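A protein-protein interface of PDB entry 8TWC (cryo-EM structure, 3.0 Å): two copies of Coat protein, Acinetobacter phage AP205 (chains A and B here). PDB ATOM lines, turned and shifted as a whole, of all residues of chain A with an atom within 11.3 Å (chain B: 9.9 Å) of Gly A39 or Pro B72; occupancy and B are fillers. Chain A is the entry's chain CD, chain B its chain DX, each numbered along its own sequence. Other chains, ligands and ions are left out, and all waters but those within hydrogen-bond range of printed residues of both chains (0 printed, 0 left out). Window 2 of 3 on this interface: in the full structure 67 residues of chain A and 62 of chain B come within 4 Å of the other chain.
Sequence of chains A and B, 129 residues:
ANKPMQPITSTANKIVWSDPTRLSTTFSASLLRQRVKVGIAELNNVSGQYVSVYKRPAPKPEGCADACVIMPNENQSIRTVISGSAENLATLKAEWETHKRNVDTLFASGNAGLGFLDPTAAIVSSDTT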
ATOM      1  N   ARG A  35      17.114 -33.340  38.511  1.00  0.00           N
ATOM      2  CA  ARG A  35      17.354 -33.220  37.079  1.00  0.00           C
ATOM      3  C   ARG A  35      16.561 -34.304  36.358  1.00  0.00           C
ATOM      4  O   ARG A  35      16.585 -35.471  36.762  1.00  0.00           O
ATOM      5  CB  ARG A  35      18.846 -33.320  36.763  1.00  0.00           C
ATOM      6  CG  ARG A  35      19.524 -34.578  37.272  1.00  0.00           C
ATOM      7  CD  ARG A  35      21.014 -34.550  36.982  1.00  0.00           C
ATOM      8  NE  ARG A  35      21.685 -33.468  37.692  1.00  0.00           N
ATOM      9  CZ  ARG A  35      22.171 -33.568  38.921  1.00  0.00           C
ATOM     10  NH1 ARG A  35      22.078 -34.692  39.614  1.00  0.00           N
ATOM     11  NH2 ARG A  35      22.764 -32.512  39.472  1.00  0.00           N
ATOM     12  N   VAL A  36      15.845 -33.913  35.306  1.00  0.00           N
ATOM     13  CA  VAL A  36      14.939 -34.802  34.589  1.00  0.00           C
ATOM     14  C   VAL A  36      15.320 -34.802  33.116  1.00  0.00           C
ATOM     15  O   VAL A  36      15.510 -33.736  32.520  1.00  0.00           O
ATOM     16  CB  VAL A  36      13.468 -34.379  34.766  1.00  0.00           C
ATOM     17  CG1 VAL A  36      12.551 -35.309  33.991  1.00  0.00           C
ATOM     18  CG2 VAL A  36      13.094 -34.359  36.240  1.00  0.00           C
ATOM     19  N   LYS A  37      15.430 -35.996  32.532  1.00  0.00           N
ATOM     20  CA  LYS A  37      15.801 -36.153  31.126  1.00  0.00           C
ATOM     21  C   LYS A  37      14.524 -36.268  30.299  1.00  0.00           C
ATOM     22  O   LYS A  37      14.021 -37.355  30.020  1.00  0.00           O
ATOM     23  CB  LYS A  37      16.708 -37.367  30.947  1.00  0.00           C
ATOM     24  CG  LYS A  37      18.083 -37.211  31.575  1.00  0.00           C
ATOM     25  CD  LYS A  37      19.049 -38.264  31.061  1.00  0.00           C
ATOM     26  CE  LYS A  37      18.726 -39.634  31.633  1.00  0.00           C
ATOM     27  NZ  LYS A  37      19.710 -40.663  31.200  1.00  0.00           N
ATOM     28  N   VAL A  38      13.994 -35.110  29.904  1.00  0.00           N
ATOM     29  CA  VAL A  38      12.758 -35.084  29.126  1.00  0.00           C
ATOM     30  C   VAL A  38      13.053 -35.244  27.640  1.00  0.00           C
ATOM     31  O   VAL A  38      12.602 -36.201  27.000  1.00  0.00           O
ATOM     32  CB  VAL A  38      11.982 -33.785  29.405  1.00  0.00           C
ATOM     33  CG1 VAL A  38      10.822 -33.643  28.433  1.00  0.00           C
ATOM     34  CG2 VAL A  38      11.487 -33.760  30.842  1.00  0.00           C
ATOM     35  N   GLY A  39      13.818 -34.317  27.076  1.00  0.00           N
ATOM     36  CA  GLY A  39      14.041 -34.248  25.645  1.00  0.00           C
ATOM     37  C   GLY A  39      15.478 -34.518  25.263  1.00  0.00           C
ATOM     38  O   GLY A  39      16.069 -33.747  24.505  1.00  0.00           O
ATOM     39  N   ILE A  40      16.059 -35.565  25.860  1.00  0.00           N
ATOM     40  CA  ILE A  40      17.469 -35.959  25.787  1.00  0.00           C
ATOM     41  C   ILE A  40      18.340 -34.776  26.195  1.00  0.00           C
ATOM     42  O   ILE A  40      19.533 -34.722  25.877  1.00  0.00           O
ATOM     43  CB  ILE A  40      17.883 -36.535  24.410  1.00  0.00           C
ATOM     44  CG1 ILE A  40      17.945 -35.490  23.293  1.00  0.00           C
ATOM     45  CG2 ILE A  40      16.940 -37.661  24.008  1.00  0.00           C
ATOM     46  CD1 ILE A  40      18.558 -36.002  22.010  1.00  0.00           C
ATOM     47  N   ALA A  41      17.744 -33.829  26.917  1.00  0.00           N
ATOM     48  CA  ALA A  41      18.454 -32.725  27.544  1.00  0.00           C
ATOM     49  C   ALA A  41      18.071 -32.699  29.015  1.00  0.00           C
ATOM     50  O   ALA A  41      16.893 -32.853  29.353  1.00  0.00           O
ATOM     51  CB  ALA A  41      18.120 -31.389  26.876  1.00  0.00           C
ATOM     52  N   GLU A  42      19.060 -32.505  29.885  1.00  0.00           N
ATOM     53  CA  GLU A  42      18.847 -32.596  31.329  1.00  0.00           C
ATOM     54  C   GLU A  42      18.315 -31.263  31.845  1.00  0.00           C
ATOM     55  O   GLU A  42      19.059 -30.341  32.187  1.00  0.00           O
ATOM     56  CB  GLU A  42      20.136 -32.993  32.035  1.00  0.00           C
ATOM     57  CG  GLU A  42      20.595 -34.411  31.737  1.00  0.00           C
ATOM     58  CD  GLU A  42      21.848 -34.789  32.501  1.00  0.00           C
ATOM     59  OE1 GLU A  42      22.422 -33.907  33.173  1.00  0.00           O
ATOM     60  OE2 GLU A  42      22.259 -35.966  32.428  1.00  0.00           O
ATOM     61  N   LEU A  43      16.989 -31.164  31.902  1.00  0.00           N
ATOM     62  CA  LEU A  43      16.355 -29.988  32.480  1.00  0.00           C
ATOM     63  C   LEU A  43      16.379 -30.073  34.000  1.00  0.00           C
ATOM     64  O   LEU A  43      16.227 -31.151  34.580  1.00  0.00           O
ATOM     65  CB  LEU A  43      14.917 -29.862  31.978  1.00  0.00           C
ATOM     66  CG  LEU A  43      14.713 -30.016  30.471  1.00  0.00           C
ATOM     67  CD1 LEU A  43      13.255 -29.804  30.105  1.00  0.00           C
ATOM     68  CD2 LEU A  43      15.602 -29.050  29.708  1.00  0.00           C
ATOM     69  N   ASN A  44      16.572 -28.925  34.648  1.00  0.00           N
ATOM     70  CA  ASN A  44      16.654 -28.868  36.108  1.00  0.00           C
ATOM     71  C   ASN A  44      15.293 -28.479  36.685  1.00  0.00           C
ATOM     72  O   ASN A  44      14.877 -27.319  36.684  1.00  0.00           O
ATOM     73  CB  ASN A  44      17.749 -27.903  36.541  1.00  0.00           C
ATOM     74  CG  ASN A  44      19.076 -28.201  35.881  1.00  0.00           C
ATOM     75  OD1 ASN A  44      19.174 -28.252  34.656  1.00  0.00           O
ATOM     76  ND2 ASN A  44      20.107 -28.407  36.691  1.00  0.00           N
ATOM     77  N   ASN A  45      14.596 -29.492  37.189  1.00  0.00           N
ATOM     78  CA  ASN A  45      13.274 -29.283  37.760  1.00  0.00           C
ATOM     79  C   ASN A  45      13.380 -28.718  39.170  1.00  0.00           C
ATOM     80  O   ASN A  45      14.248 -29.112  39.953  1.00  0.00           O
ATOM     81  CB  ASN A  45      12.491 -30.595  37.777  1.00  0.00           C
ATOM     82  CG  ASN A  45      11.030 -30.399  38.127  1.00  0.00           C
ATOM     83  OD1 ASN A  45      10.570 -29.276  38.326  1.00  0.00           O
ATOM     84  ND2 ASN A  45      10.291 -31.499  38.207  1.00  0.00           N
ATOM     85  N   SER A  85      10.521 -26.845  35.134  1.00  0.00           N
ATOM     86  CA  SER A  85      11.927 -26.641  34.819  1.00  0.00           C
ATOM     87  C   SER A  85      12.309 -25.178  34.994  1.00  0.00           C
ATOM     88  O   SER A  85      11.506 -24.274  34.752  1.00  0.00           O
ATOM     89  CB  SER A  85      12.225 -27.091  33.390  1.00  0.00           C
ATOM     90  OG  SER A  85      11.556 -26.270  32.450  1.00  0.00           O
ATOM     91  N   GLU A  87      14.277 -23.573  33.196  1.00  0.00           N
ATOM     92  CA  GLU A  87      14.503 -22.930  31.907  1.00  0.00           C
ATOM     93  C   GLU A  87      13.233 -22.297  31.352  1.00  0.00           C
ATOM     94  O   GLU A  87      13.304 -21.444  30.460  1.00  0.00           O
ATOM     95  CB  GLU A  87      15.074 -23.945  30.918  1.00  0.00           C
ATOM     96  CG  GLU A  87      16.474 -24.419  31.276  1.00  0.00           C
ATOM     97  CD  GLU A  87      17.020 -25.440  30.298  1.00  0.00           C
ATOM     98  OE1 GLU A  87      16.264 -25.875  29.405  1.00  0.00           O
ATOM     99  OE2 GLU A  87      18.207 -25.807  30.421  1.00  0.00           O
ATOM    100  N   ASN A  88      12.071 -22.694  31.860  1.00  0.00           N
ATOM    101  CA  ASN A  88      10.782 -22.158  31.437  1.00  0.00           C
ATOM    102  C   ASN A  88      10.142 -21.338  32.553  1.00  0.00           C
ATOM    103  O   ASN A  88       8.935 -21.420  32.804  1.00  0.00           O
ATOM    104  CB  ASN A  88       9.854 -23.278  30.978  1.00  0.00           C
ATOM    105  CG  ASN A  88      10.168 -23.752  29.575  1.00  0.00           C
ATOM    106  OD1 ASN A  88      10.297 -24.949  29.326  1.00  0.00           O
ATOM    107  ND2 ASN A  88      10.294 -22.811  28.649  1.00  0.00           N
ATOM    108  N   LYS B  55       1.307 -28.652  29.837  1.00  0.00           N
ATOM    109  CA  LYS B  55       2.436 -29.365  29.256  1.00  0.00           C
ATOM    110  C   LYS B  55       3.115 -28.451  28.243  1.00  0.00           C
ATOM    111  O   LYS B  55       2.653 -28.316  27.106  1.00  0.00           O
ATOM    112  CB  LYS B  55       1.982 -30.677  28.622  1.00  0.00           C
ATOM    113  CG  LYS B  55       1.636 -31.733  29.654  1.00  0.00           C
ATOM    114  CD  LYS B  55       1.256 -33.054  29.021  1.00  0.00           C
ATOM    115  CE  LYS B  55       0.940 -34.083  30.092  1.00  0.00           C
ATOM    116  NZ  LYS B  55       0.471 -35.370  29.513  1.00  0.00           N
ATOM    117  N   ARG B  56       4.212 -27.826  28.664  1.00  0.00           N
ATOM    118  CA  ARG B  56       4.935 -26.845  27.876  1.00  0.00           C
ATOM    119  C   ARG B  56       6.085 -27.506  27.139  1.00  0.00           C
ATOM    120  O   ARG B  56       6.805 -28.321  27.733  1.00  0.00           O
ATOM    121  CB  ARG B  56       5.468 -25.727  28.777  1.00  0.00           C
ATOM    122  CG  ARG B  56       5.976 -24.509  28.032  1.00  0.00           C
ATOM    123  CD  ARG B  56       4.842 -23.563  27.696  1.00  0.00           C
ATOM    124  NE  ARG B  56       4.196 -23.044  28.895  1.00  0.00           N
ATOM    125  CZ  ARG B  56       3.267 -22.097  28.893  1.00  0.00           C
ATOM    126  NH1 ARG B  56       2.853 -21.539  27.768  1.00  0.00           N
ATOM    127  NH2 ARG B  56       2.742 -21.702  30.049  1.00  0.00           N
ATOM    128  N   PRO B  57       6.285 -27.198  25.860  1.00  0.00           N
ATOM    129  CA  PRO B  57       7.439 -27.748  25.144  1.00  0.00           C
ATOM    130  C   PRO B  57       8.748 -27.271  25.749  1.00  0.00           C
ATOM    131  O   PRO B  57       8.854 -26.155  26.265  1.00  0.00           O
ATOM    132  CB  PRO B  57       7.258 -27.211  23.719  1.00  0.00           C
ATOM    133  CG  PRO B  57       5.804 -26.875  23.623  1.00  0.00           C
ATOM    134  CD  PRO B  57       5.436 -26.379  24.983  1.00  0.00           C
ATOM    135  N   ALA B  58       9.752 -28.141  25.685  1.00  0.00           N
ATOM    136  CA  ALA B  58      11.068 -27.787  26.185  1.00  0.00           C
ATOM    137  C   ALA B  58      11.643 -26.643  25.353  1.00  0.00           C
ATOM    138  O   ALA B  58      11.344 -26.521  24.162  1.00  0.00           O
ATOM    139  CB  ALA B  58      11.998 -28.998  26.143  1.00  0.00           C
ATOM    140  N   PRO B  59      12.458 -25.775  25.958  1.00  0.00           N
ATOM    141  CA  PRO B  59      12.921 -24.580  25.238  1.00  0.00           C
ATOM    142  C   PRO B  59      13.808 -24.904  24.049  1.00  0.00           C
ATOM    143  O   PRO B  59      14.719 -25.732  24.141  1.00  0.00           O
ATOM    144  CB  PRO B  59      13.688 -23.800  26.313  1.00  0.00           C
ATOM    145  CG  PRO B  59      14.093 -24.823  27.306  1.00  0.00           C
ATOM    146  CD  PRO B  59      12.994 -25.838  27.327  1.00  0.00           C
ATOM    147  N   LYS B  60      13.540 -24.248  22.925  1.00  0.00           N
ATOM    148  CA  LYS B  60      14.336 -24.389  21.714  1.00  0.00           C
ATOM    149  C   LYS B  60      15.687 -23.712  21.908  1.00  0.00           C
ATOM    150  O   LYS B  60      15.806 -22.798  22.733  1.00  0.00           O
ATOM    151  CB  LYS B  60      13.587 -23.796  20.519  1.00  0.00           C
ATOM    152  CG  LYS B  60      13.384 -22.291  20.600  1.00  0.00           C
ATOM    153  CD  LYS B  60      12.875 -21.725  19.285  1.00  0.00           C
ATOM    154  CE  LYS B  60      13.948 -21.770  18.213  1.00  0.00           C
ATOM    155  NZ  LYS B  60      13.497 -21.144  16.940  1.00  0.00           N
ATOM    156  N   PRO B  61      16.730 -24.141  21.187  1.00  0.00           N
ATOM    157  CA  PRO B  61      18.033 -23.471  21.305  1.00  0.00           C
ATOM    158  C   PRO B  61      17.961 -21.996  20.945  1.00  0.00           C
ATOM    159  O   PRO B  61      17.234 -21.608  20.026  1.00  0.00           O
ATOM    160  CB  PRO B  61      18.919 -24.254  20.326  1.00  0.00           C
ATOM    161  CG  PRO B  61      17.959 -24.951  19.413  1.00  0.00           C
ATOM    162  CD  PRO B  61      16.790 -25.291  20.273  1.00  0.00           C
ATOM    163  N   VAL B  69      10.713 -27.333  14.395  1.00  0.00           N
ATOM    164  CA  VAL B  69      11.415 -28.411  15.083  1.00  0.00           C
ATOM    165  C   VAL B  69      10.824 -28.514  16.481  1.00  0.00           C
ATOM    166  O   VAL B  69      11.024 -27.624  17.317  1.00  0.00           O
ATOM    167  CB  VAL B  69      12.933 -28.170  15.131  1.00  0.00           C
ATOM    168  CG1 VAL B  69      13.594 -29.143  16.095  1.00  0.00           C
ATOM    169  CG2 VAL B  69      13.537 -28.306  13.743  1.00  0.00           C
ATOM    170  N   ILE B  70      10.089 -29.590  16.745  1.00  0.00           N
ATOM    171  CA  ILE B  70       9.322 -29.729  17.978  1.00  0.00           C
ATOM    172  C   ILE B  70      10.017 -30.742  18.876  1.00  0.00           C
ATOM    173  O   ILE B  70      10.385 -31.832  18.424  1.00  0.00           O
ATOM    174  CB  ILE B  70       7.861 -30.135  17.707  1.00  0.00           C
ATOM    175  CG1 ILE B  70       7.085 -30.262  19.022  1.00  0.00           C
ATOM    176  CG2 ILE B  70       7.784 -31.411  16.875  1.00  0.00           C
ATOM    177  CD1 ILE B  70       5.599 -30.475  18.835  1.00  0.00           C
ATOM    178  N   MET B  71      10.216 -30.371  20.139  1.00  0.00           N
ATOM    179  CA  MET B  71      10.828 -31.233  21.140  1.00  0.00           C
ATOM    180  C   MET B  71       9.808 -31.534  22.235  1.00  0.00           C
ATOM    181  O   MET B  71       8.873 -30.749  22.434  1.00  0.00           O
ATOM    182  CB  MET B  71      12.095 -30.575  21.691  1.00  0.00           C
ATOM    183  CG  MET B  71      11.870 -29.285  22.444  1.00  0.00           C
ATOM    184  SD  MET B  71      13.449 -28.573  22.938  1.00  0.00           S
ATOM    185  CE  MET B  71      14.046 -27.980  21.360  1.00  0.00           C
ATOM    186  N   PRO B  72       9.943 -32.645  22.955  1.00  0.00           N
ATOM    187  CA  PRO B  72       8.838 -33.137  23.785  1.00  0.00           C
ATOM    188  C   PRO B  72       8.496 -32.194  24.931  1.00  0.00           C
ATOM    189  O   PRO B  72       9.281 -31.338  25.340  1.00  0.00           O
ATOM    190  CB  PRO B  72       9.358 -34.479  24.313  1.00  0.00           C
ATOM    191  CG  PRO B  72      10.827 -34.380  24.217  1.00  0.00           C
ATOM    192  CD  PRO B  72      11.103 -33.551  23.005  1.00  0.00           C
ATOM    193  N   ASN B  73       7.283 -32.378  25.446  1.00  0.00           N
ATOM    194  CA  ASN B  73       6.702 -31.512  26.455  1.00  0.00           C
ATOM    195  C   ASN B  73       7.184 -31.903  27.850  1.00  0.00           C
ATOM    196  O   ASN B  73       7.654 -33.018  28.089  1.00  0.00           O
ATOM    197  CB  ASN B  73       5.177 -31.581  26.393  1.00  0.00           C
ATOM    198  CG  ASN B  73       4.615 -30.931  25.146  1.00  0.00           C
ATOM    199  OD1 ASN B  73       5.067 -29.868  24.727  1.00  0.00           O
ATOM    200  ND2 ASN B  73       3.620 -31.572  24.545  1.00  0.00           N
ATOM    201  N   GLU B  74       7.057 -30.960  28.782  1.00  0.00           N
ATOM    202  CA  GLU B  74       7.385 -31.186  30.183  1.00  0.00           C
ATOM    203  C   GLU B  74       6.153 -30.891  31.021  1.00  0.00           C
ATOM    204  O   GLU B  74       5.275 -30.137  30.592  1.00  0.00           O
ATOM    205  CB  GLU B  74       8.548 -30.304  30.637  1.00  0.00           C
ATOM    206  CG  GLU B  74       8.221 -28.826  30.652  1.00  0.00           C
ATOM    207  CD  GLU B  74       9.409 -27.980  31.037  1.00  0.00           C
ATOM    208  OE1 GLU B  74      10.494 -28.555  31.256  1.00  0.00           O
ATOM    209  OE2 GLU B  74       9.256 -26.745  31.138  1.00  0.00           O
ATOM    210  N   ASN B  75       6.088 -31.483  32.210  1.00  0.00           N
ATOM    211  CA  ASN B  75       4.927 -31.305  33.070  1.00  0.00           C
ATOM    212  C   ASN B  75       5.132 -30.097  33.977  1.00  0.00           C
ATOM    213  O   ASN B  75       6.110 -30.033  34.730  1.00  0.00           O
ATOM    214  CB  ASN B  75       4.691 -32.566  33.897  1.00  0.00           C
ATOM    215  CG  ASN B  75       3.451 -32.473  34.771  1.00  0.00           C
ATOM    216  OD1 ASN B  75       2.662 -31.535  34.657  1.00  0.00           O
ATOM    217  ND2 ASN B  75       3.278 -33.451  35.652  1.00  0.00           N
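Among the printed residues, pairs that only touch across the chains: Glu A87 with Pro B59 (3.2 Å), Leu A43 with Glu B74 (3.2 Å), Val A38 with Asn B73 (3.2 Å), Asn A88 with Pro B59 (3.5 Å), Gly A39 with Pro B72 (3.5 Å), Asn A88 with Pro B57 (3.6 Å) and Val A38 with Pro B72 (3.8 Å).
The side-chain carboxylate of Glu B74 is in hydrogen-bond range of the side-chain hydroxyl of Ser A85 (2.7 Å). The side-chain amide oxygen (OD1) of Asn A88 sits close to the side-chain carboxylate (OE2) of Glu B74 (2.8 Å).
N of Val A36 is in hydrogen-bond range of O of Leu A43 (2.9 Å). O of Arg B56 is in hydrogen-bond range of N of Glu B74 (2.9 Å). O of Pro B72 sits at hydrogen-bond distance from N of Ala B58, at 3.2 Å.
Of the printed residues of chain B, Gly A39 touches Pro B72. Of chain A, only Val A38 (3.8 Å) and Gly A39 (3.5 Å) come within 4 Å of Pro B72. Of chain B, only Pro B72 (3.8 Å) and Asn B73 (3.2 Å) come within 4 Å of Val A38. No residue of chain B comes within 4 Å of Ile A40. No residue of chain B comes within 4 Å of Ala A41. Of chain A, only Asn A88 (3.6 Å) comes within 4 Å of Pro B57. No residue of chain A comes within 4 Å of Ala B58. No residue of chain A comes within 4 Å of Ile B70. Of chain A, only Val A38 (3.2 Å) comes within 4 Å of Asn B73. Printed residues of chain B within 4 Å of Ser A85: Glu B74 (2.7 Å). Of the printed residues of chain B, Leu A43 touches Glu B74 (3.2 Å). The nearest printed residue of chain B that does not touch Ser A85 is Pro B59 (5.3 Å).
No position is printed for both chains. Of the 9 pairs that touch across the chains among the printed residues, none has its exchanged pair printed and touching as well.
Of the 14 printed residues of chain B, 5 touch a printed residue of chain A. Printed residues of chain B that touch a printed residue of chain A: Pro B57, Pro B59, Pro B72, Asn B73 and Glu B74. Printed residues of chain A that touch a printed residue of chain B: Val A38, Gly A39, Leu A43, Ser A85, Glu A87 and Asn A88.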
